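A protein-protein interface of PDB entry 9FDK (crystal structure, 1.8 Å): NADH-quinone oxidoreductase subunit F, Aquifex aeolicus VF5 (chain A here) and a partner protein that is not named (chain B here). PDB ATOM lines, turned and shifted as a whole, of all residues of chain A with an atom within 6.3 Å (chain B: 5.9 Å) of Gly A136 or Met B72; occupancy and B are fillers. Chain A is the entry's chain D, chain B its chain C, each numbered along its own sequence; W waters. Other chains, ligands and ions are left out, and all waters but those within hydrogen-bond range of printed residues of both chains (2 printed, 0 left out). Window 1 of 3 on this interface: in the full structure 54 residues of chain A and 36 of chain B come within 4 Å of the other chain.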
ATOM      1  N   ASP A  94     -15.017  -1.267  19.145  1.00  0.00           N
ATOM      2  CA  ASP A  94     -15.174  -0.162  18.213  1.00  0.00           C
ATOM      3  C   ASP A  94     -15.491  -0.627  16.785  1.00  0.00           C
ATOM      4  O   ASP A  94     -15.871   0.194  15.958  1.00  0.00           O
ATOM      5  CB  ASP A  94     -13.966   0.768  18.170  1.00  0.00           C
ATOM      6  CG  ASP A  94     -14.361   2.146  17.674  1.00  0.00           C
ATOM      7  OD1 ASP A  94     -15.258   2.736  18.308  1.00  0.00           O
ATOM      8  OD2 ASP A  94     -13.888   2.552  16.579  1.00  0.00           O
ATOM      9  N   ILE A 134     -17.597   0.829  22.982  1.00  0.00           N
ATOM     10  CA  ILE A 134     -18.397   0.339  21.870  1.00  0.00           C
ATOM     11  C   ILE A 134     -18.711   1.515  20.959  1.00  0.00           C
ATOM     12  O   ILE A 134     -19.099   2.589  21.423  1.00  0.00           O
ATOM     13  CB  ILE A 134     -19.655  -0.412  22.339  1.00  0.00           C
ATOM     14  CG1 ILE A 134     -20.405  -1.065  21.177  1.00  0.00           C
ATOM     15  CG2 ILE A 134     -20.593   0.466  23.164  1.00  0.00           C
ATOM     16  CD1 ILE A 134     -21.479  -2.046  21.622  1.00  0.00           C
ATOM     17  N   ARG A 135     -18.585   1.275  19.652  1.00  0.00           N
ATOM     18  CA  ARG A 135     -18.809   2.334  18.685  1.00  0.00           C
ATOM     19  C   ARG A 135     -20.220   2.868  18.894  1.00  0.00           C
ATOM     20  O   ARG A 135     -21.131   2.135  19.300  1.00  0.00           O
ATOM     21  CB  ARG A 135     -18.616   1.836  17.254  1.00  0.00           C
ATOM     22  CG  ARG A 135     -19.607   0.745  16.857  1.00  0.00           C
ATOM     23  CD  ARG A 135     -19.309   0.291  15.434  1.00  0.00           C
ATOM     24  NE  ARG A 135     -19.579   1.346  14.455  1.00  0.00           N
ATOM     25  CZ  ARG A 135     -19.550   1.198  13.140  1.00  0.00           C
ATOM     26  NH1 ARG A 135     -19.234   0.029  12.617  1.00  0.00           N
ATOM     27  NH2 ARG A 135     -19.814   2.238  12.356  1.00  0.00           N
ATOM     28  N   GLY A 136     -20.373   4.163  18.618  1.00  0.00           N
ATOM     29  CA  GLY A 136     -21.629   4.873  18.776  1.00  0.00           C
ATOM     30  C   GLY A 136     -22.746   4.341  17.879  1.00  0.00           C
ATOM     31  O   GLY A 136     -23.898   4.460  18.259  1.00  0.00           O
ATOM     32  N   GLU A 137     -22.398   3.713  16.749  1.00  0.00           N
ATOM     33  CA  GLU A 137     -23.379   3.197  15.802  1.00  0.00           C
ATOM     34  C   GLU A 137     -23.846   1.781  16.157  1.00  0.00           C
ATOM     35  O   GLU A 137     -24.612   1.186  15.387  1.00  0.00           O
ATOM     36  CB  GLU A 137     -22.866   3.253  14.364  1.00  0.00           C
ATOM     37  CG  GLU A 137     -22.356   4.628  13.941  1.00  0.00           C
ATOM     38  CD  GLU A 137     -20.901   4.927  14.290  1.00  0.00           C
ATOM     39  OE1 GLU A 137     -20.232   4.185  15.052  1.00  0.00           O
ATOM     40  OE2 GLU A 137     -20.436   5.957  13.749  1.00  0.00           O
ATOM     41  N   TYR A 138     -23.452   1.271  17.337  1.00  0.00           N
ATOM     42  CA  TYR A 138     -24.001   0.032  17.884  1.00  0.00           C
ATOM     43  C   TYR A 138     -24.830   0.336  19.132  1.00  0.00           C
ATOM     44  O   TYR A 138     -24.486  -0.065  20.254  1.00  0.00           O
ATOM     45  CB  TYR A 138     -22.891  -0.963  18.229  1.00  0.00           C
ATOM     46  CG  TYR A 138     -22.154  -1.696  17.113  1.00  0.00           C
ATOM     47  CD1 TYR A 138     -22.613  -1.700  15.795  1.00  0.00           C
ATOM     48  CD2 TYR A 138     -21.037  -2.465  17.407  1.00  0.00           C
ATOM     49  CE1 TYR A 138     -21.943  -2.393  14.798  1.00  0.00           C
ATOM     50  CE2 TYR A 138     -20.382  -3.196  16.426  1.00  0.00           C
ATOM     51  CZ  TYR A 138     -20.838  -3.160  15.119  1.00  0.00           C
ATOM     52  OH  TYR A 138     -20.186  -3.858  14.149  1.00  0.00           O
ATOM     53  N   PRO A 139     -25.947   1.081  19.022  1.00  0.00           N
ATOM     54  CA  PRO A 139     -26.723   1.445  20.214  1.00  0.00           C
ATOM     55  C   PRO A 139     -27.387   0.251  20.895  1.00  0.00           C
ATOM     56  O   PRO A 139     -27.487   0.207  22.120  1.00  0.00           O
ATOM     57  CB  PRO A 139     -27.736   2.466  19.678  1.00  0.00           C
ATOM     58  CG  PRO A 139     -27.884   2.094  18.216  1.00  0.00           C
ATOM     59  CD  PRO A 139     -26.501   1.648  17.787  1.00  0.00           C
ATOM     60  N   ARG A 175     -19.282   4.866  25.013  1.00  0.00           N
ATOM     61  CA  ARG A 175     -19.736   4.871  23.629  1.00  0.00           C
ATOM     62  C   ARG A 175     -18.837   5.795  22.802  1.00  0.00           C
ATOM     63  O   ARG A 175     -18.488   6.889  23.239  1.00  0.00           O
ATOM     64  CB  ARG A 175     -21.174   5.378  23.508  1.00  0.00           C
ATOM     65  CG  ARG A 175     -22.230   4.447  24.078  1.00  0.00           C
ATOM     66  CD  ARG A 175     -23.634   4.969  23.880  1.00  0.00           C
ATOM     67  NE  ARG A 175     -24.058   4.833  22.483  1.00  0.00           N
ATOM     68  CZ  ARG A 175     -25.106   5.438  21.946  1.00  0.00           C
ATOM     69  NH1 ARG A 175     -25.826   6.274  22.678  1.00  0.00           N
ATOM     70  NH2 ARG A 175     -25.420   5.221  20.677  1.00  0.00           N
ATOM     71  N   GLY A 176     -18.453   5.331  21.615  1.00  0.00           N
ATOM     72  CA  GLY A 176     -17.875   6.183  20.585  1.00  0.00           C
ATOM     73  C   GLY A 176     -18.908   7.127  19.981  1.00  0.00           C
ATOM     74  O   GLY A 176     -20.068   7.157  20.397  1.00  0.00           O
ATOM     75  N   ALA A 177     -18.454   7.929  19.016  1.00  0.00           N
ATOM     76  CA  ALA A 177     -19.305   8.938  18.404  1.00  0.00           C
ATOM     77  C   ALA A 177     -18.894   9.211  16.952  1.00  0.00           C
ATOM     78  O   ALA A 177     -19.077  10.321  16.447  1.00  0.00           O
ATOM     79  CB  ALA A 177     -19.269  10.190  19.248  1.00  0.00           C
ATOM     80  N   GLY A 178     -18.379   8.179  16.273  1.00  0.00           N
ATOM     81  CA  GLY A 178     -18.345   8.160  14.821  1.00  0.00           C
ATOM     82  C   GLY A 178     -16.950   8.080  14.199  1.00  0.00           C
ATOM     83  O   GLY A 178     -16.829   8.219  12.984  1.00  0.00           O
ATOM     84  N   ALA A 179     -15.909   7.795  14.980  1.00  0.00           N
ATOM     85  CA  ALA A 179     -14.544   7.827  14.472  1.00  0.00           C
ATOM     86  C   ALA A 179     -13.927   6.437  14.458  1.00  0.00           C
ATOM     87  O   ALA A 179     -13.735   5.825  15.520  1.00  0.00           O
ATOM     88  CB  ALA A 179     -13.732   8.759  15.339  1.00  0.00           C
ATOM     89  N   HIS B  35     -24.286  12.688  23.261  1.00  0.00           N
ATOM     90  CA  HIS B  35     -25.328  11.831  22.712  1.00  0.00           C
ATOM     91  C   HIS B  35     -26.683  12.185  23.330  1.00  0.00           C
ATOM     92  O   HIS B  35     -27.680  12.301  22.630  1.00  0.00           O
ATOM     93  CB  HIS B  35     -25.007  10.350  22.946  1.00  0.00           C
ATOM     94  CG  HIS B  35     -24.017   9.763  22.003  1.00  0.00           C
ATOM     95  ND1 HIS B  35     -24.223   9.715  20.641  1.00  0.00           N
ATOM     96  CD2 HIS B  35     -22.864   9.108  22.230  1.00  0.00           C
ATOM     97  CE1 HIS B  35     -23.207   9.077  20.073  1.00  0.00           C
ATOM     98  NE2 HIS B  35     -22.365   8.699  21.021  1.00  0.00           N
ATOM     99  N   GLN B  38     -28.003  15.519  21.947  1.00  0.00           N
ATOM    100  CA  GLN B  38     -28.443  15.419  20.564  1.00  0.00           C
ATOM    101  C   GLN B  38     -29.752  14.640  20.500  1.00  0.00           C
ATOM    102  O   GLN B  38     -30.634  14.981  19.713  1.00  0.00           O
ATOM    103  CB  GLN B  38     -27.393  14.775  19.659  1.00  0.00           C
ATOM    104  CG  GLN B  38     -27.829  14.629  18.204  1.00  0.00           C
ATOM    105  CD  GLN B  38     -26.671  14.741  17.235  1.00  0.00           C
ATOM    106  OE1 GLN B  38     -25.941  15.734  17.237  1.00  0.00           O
ATOM    107  NE2 GLN B  38     -26.444  13.706  16.435  1.00  0.00           N
ATOM    108  N   TYR B  70     -16.024  14.392  16.343  1.00  0.00           N
ATOM    109  CA  TYR B  70     -16.814  13.170  16.274  1.00  0.00           C
ATOM    110  C   TYR B  70     -17.994  13.350  15.316  1.00  0.00           C
ATOM    111  O   TYR B  70     -18.891  14.151  15.561  1.00  0.00           O
ATOM    112  CB  TYR B  70     -17.234  12.789  17.697  1.00  0.00           C
ATOM    113  CG  TYR B  70     -16.092  12.270  18.559  1.00  0.00           C
ATOM    114  CD1 TYR B  70     -15.625  10.971  18.414  1.00  0.00           C
ATOM    115  CD2 TYR B  70     -15.484  13.070  19.516  1.00  0.00           C
ATOM    116  CE1 TYR B  70     -14.607  10.475  19.213  1.00  0.00           C
ATOM    117  CE2 TYR B  70     -14.446  12.596  20.301  1.00  0.00           C
ATOM    118  CZ  TYR B  70     -14.011  11.292  20.158  1.00  0.00           C
ATOM    119  OH  TYR B  70     -12.994  10.822  20.947  1.00  0.00           O
ATOM    120  N   ASP B  71     -17.999  12.539  14.254  1.00  0.00           N
ATOM    121  CA  ASP B  71     -18.876  12.719  13.110  1.00  0.00           C
ATOM    122  C   ASP B  71     -20.351  12.494  13.443  1.00  0.00           C
ATOM    123  O   ASP B  71     -21.203  12.954  12.690  1.00  0.00           O
ATOM    124  CB  ASP B  71     -18.481  11.797  11.963  1.00  0.00           C
ATOM    125  CG  ASP B  71     -17.275  12.251  11.146  1.00  0.00           C
ATOM    126  OD1 ASP B  71     -16.778  13.388  11.373  1.00  0.00           O
ATOM    127  OD2 ASP B  71     -16.819  11.459  10.295  1.00  0.00           O
ATOM    128  N   MET B  72     -20.676  11.765  14.521  1.00  0.00           N
ATOM    129  CA  MET B  72     -22.081  11.505  14.810  1.00  0.00           C
ATOM    130  C   MET B  72     -22.789  12.790  15.247  1.00  0.00           C
ATOM    131  O   MET B  72     -23.990  12.897  15.059  1.00  0.00           O
ATOM    132  CB  MET B  72     -22.283  10.416  15.870  1.00  0.00           C
ATOM    133  CG  MET B  72     -21.995   9.004  15.377  1.00  0.00           C
ATOM    134  SD  MET B  72     -22.434   7.719  16.569  1.00  0.00           S
ATOM    135  CE  MET B  72     -24.226   7.761  16.604  1.00  0.00           C
ATOM    136  N   PHE B  73     -22.060  13.760  15.829  1.00  0.00           N
ATOM    137  CA  PHE B  73     -22.671  14.963  16.369  1.00  0.00           C
ATOM    138  C   PHE B  73     -22.868  15.993  15.264  1.00  0.00           C
ATOM    139  O   PHE B  73     -22.024  16.121  14.378  1.00  0.00           O
ATOM    140  CB  PHE B  73     -21.839  15.534  17.520  1.00  0.00           C
ATOM    141  CG  PHE B  73     -21.581  14.549  18.653  1.00  0.00           C
ATOM    142  CD1 PHE B  73     -22.613  13.768  19.170  1.00  0.00           C
ATOM    143  CD2 PHE B  73     -20.299  14.391  19.179  1.00  0.00           C
ATOM    144  CE1 PHE B  73     -22.364  12.840  20.174  1.00  0.00           C
ATOM    145  CE2 PHE B  73     -20.065  13.497  20.211  1.00  0.00           C
ATOM    146  CZ  PHE B  73     -21.095  12.712  20.695  1.00  0.00           C
ATOM    147  N   ASP B  74     -23.987  16.728  15.352  1.00  0.00           N
ATOM    148  CA  ASP B  74     -24.433  17.660  14.326  1.00  0.00           C
ATOM    149  C   ASP B  74     -24.828  18.969  15.007  1.00  0.00           C
ATOM    150  O   ASP B  74     -25.800  19.012  15.759  1.00  0.00           O
ATOM    151  CB  ASP B  74     -25.580  17.059  13.525  1.00  0.00           C
ATOM    152  CG  ASP B  74     -26.118  17.848  12.340  1.00  0.00           C
ATOM    153  OD1 ASP B  74     -25.721  19.017  12.158  1.00  0.00           O
ATOM    154  OD2 ASP B  74     -26.946  17.274  11.589  1.00  0.00           O
ATOM    155  N   ARG B  82     -32.681  10.754  12.186  1.00  0.00           N
ATOM    156  CA  ARG B  82     -31.545  10.689  11.281  1.00  0.00           C
ATOM    157  C   ARG B  82     -31.536   9.342  10.577  1.00  0.00           C
ATOM    158  O   ARG B  82     -31.468   8.296  11.229  1.00  0.00           O
ATOM    159  CB  ARG B  82     -30.225  10.908  12.019  1.00  0.00           C
ATOM    160  CG  ARG B  82     -30.053  12.357  12.442  1.00  0.00           C
ATOM    161  CD  ARG B  82     -29.004  12.537  13.532  1.00  0.00           C
ATOM    162  NE  ARG B  82     -29.122  13.905  14.052  1.00  0.00           N
ATOM    163  CZ  ARG B  82     -28.663  14.945  13.399  1.00  0.00           C
ATOM    164  NH1 ARG B  82     -27.778  14.766  12.437  1.00  0.00           N
ATOM    165  NH2 ARG B  82     -29.032  16.159  13.740  1.00  0.00           N
ATOM    166  N   ARG B  84     -29.292   7.216   8.696  1.00  0.00           N
ATOM    167  CA  ARG B  84     -27.879   7.017   8.410  1.00  0.00           C
ATOM    168  C   ARG B  84     -27.763   5.975   7.307  1.00  0.00           C
ATOM    169  O   ARG B  84     -28.206   4.840   7.478  1.00  0.00           O
ATOM    170  CB  ARG B  84     -27.093   6.613   9.660  1.00  0.00           C
ATOM    171  CG  ARG B  84     -26.857   7.770  10.618  1.00  0.00           C
ATOM    172  CD  ARG B  84     -26.195   7.396  11.931  1.00  0.00           C
ATOM    173  NE  ARG B  84     -25.801   8.609  12.653  1.00  0.00           N
ATOM    174  CZ  ARG B  84     -26.478   9.179  13.643  1.00  0.00           C
ATOM    175  NH1 ARG B  84     -25.989  10.278  14.208  1.00  0.00           N
ATOM    176  NH2 ARG B  84     -27.640   8.668  14.048  1.00  0.00           N
HETATM  177  O   HOH W   1     -15.330  11.215  13.751  1.00  0.00           O
HETATM  178  O   HOH W   2     -14.490  10.217  11.443  1.00  0.00           O
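Water W2 bridges the side-chain carboxylate (OD2) of Asp B71 and the backbone carbonyl oxygen (O) of Gly A178.
Water W1 lies within hydrogen-bond range of the backbone NH (N) of Asp B71 (3.0 Å) and the backbone carbonyl oxygen (O) of Gly A178 (3.4 Å).
The backbone carbonyl oxygen (O) of Gly A176 sits at hydrogen-bond distance from a ring nitrogen (NE2) of His B35.
N of Met B72 sits at hydrogen-bond distance from O of Ala A177 (2.9 Å).
N of Asp B71 is in hydrogen-bond range of O of Ala A177 (3.3 Å).
Of the 9 printed residues of chain B, 5 touch a printed residue of chain A.
Of the 12 printed residues of chain A, 6 touch a printed residue of chain B.
Among the printed residues, no Asp or Glu carboxylate lies within 4 Å of a Lys or Arg side-chain nitrogen of the other chain.
N of Gly A176 sits at hydrogen-bond distance from O of Ile A134, 2.8 Å away.
NH2 of Arg A175 is in hydrogen-bond range of O of Gly A136 (3.0 Å).
O of Met B72 is in hydrogen-bond range of NH1 of Arg B84 (3.4 Å).
The side-chain carboxylate of Glu A137 is in salt-bridge range of the guanidinium group of Arg A135, 3.0 Å away.
The backbone carbonyl oxygen of Met B72 sits at hydrogen-bond distance from the side-chain amide nitrogen of Gln B38 (2.9 Å).
The backbone NH (N) of Gly A136 sits close to the backbone carbonyl oxygen (O) of Gly A176 (3.5 Å).
Met B72 touches just these residues of chain A: Gly A136 (3.6 Å), Glu A137 (3.8 Å), Ala A177 (2.9 Å) and Gly A178 (3.8 Å).
Printed residues of chain B within 4 Å of Arg A175: His B35 (3.99 Å).
Printed residues of chain B within 4 Å of Ala A177: His B35, Tyr B70, Asp B71, Met B72 and Phe B73.
Printed residues of chain B within 4 Å of Gly A176: His B35.
Printed residues of chain B within 4 Å of Gly A178: Met B72.
Asp A94 touches none of the printed residues of chain B.
Arg A135 touches none of the printed residues of chain B.
The nearest residue of chain B that does not touch Gly A136 is His B35 (4.5 Å).
The nearest printed residue of chain A that does not touch Tyr B70 is Ala A179 (4.2 Å).
Among the printed residues, merely in contact across the chains: Gly A136 with Met B72 (3.6 Å), Glu A137 with Met B72 (3.8 Å), Arg A175 with His B35 (3.99 Å), Ala A177 with His B35 (3.9 Å), Ala A177 with Tyr B70 (3.3 Å), Ala A177 with Phe B73 (3.4 Å) and Gly A178 with Met B72 (3.8 Å).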
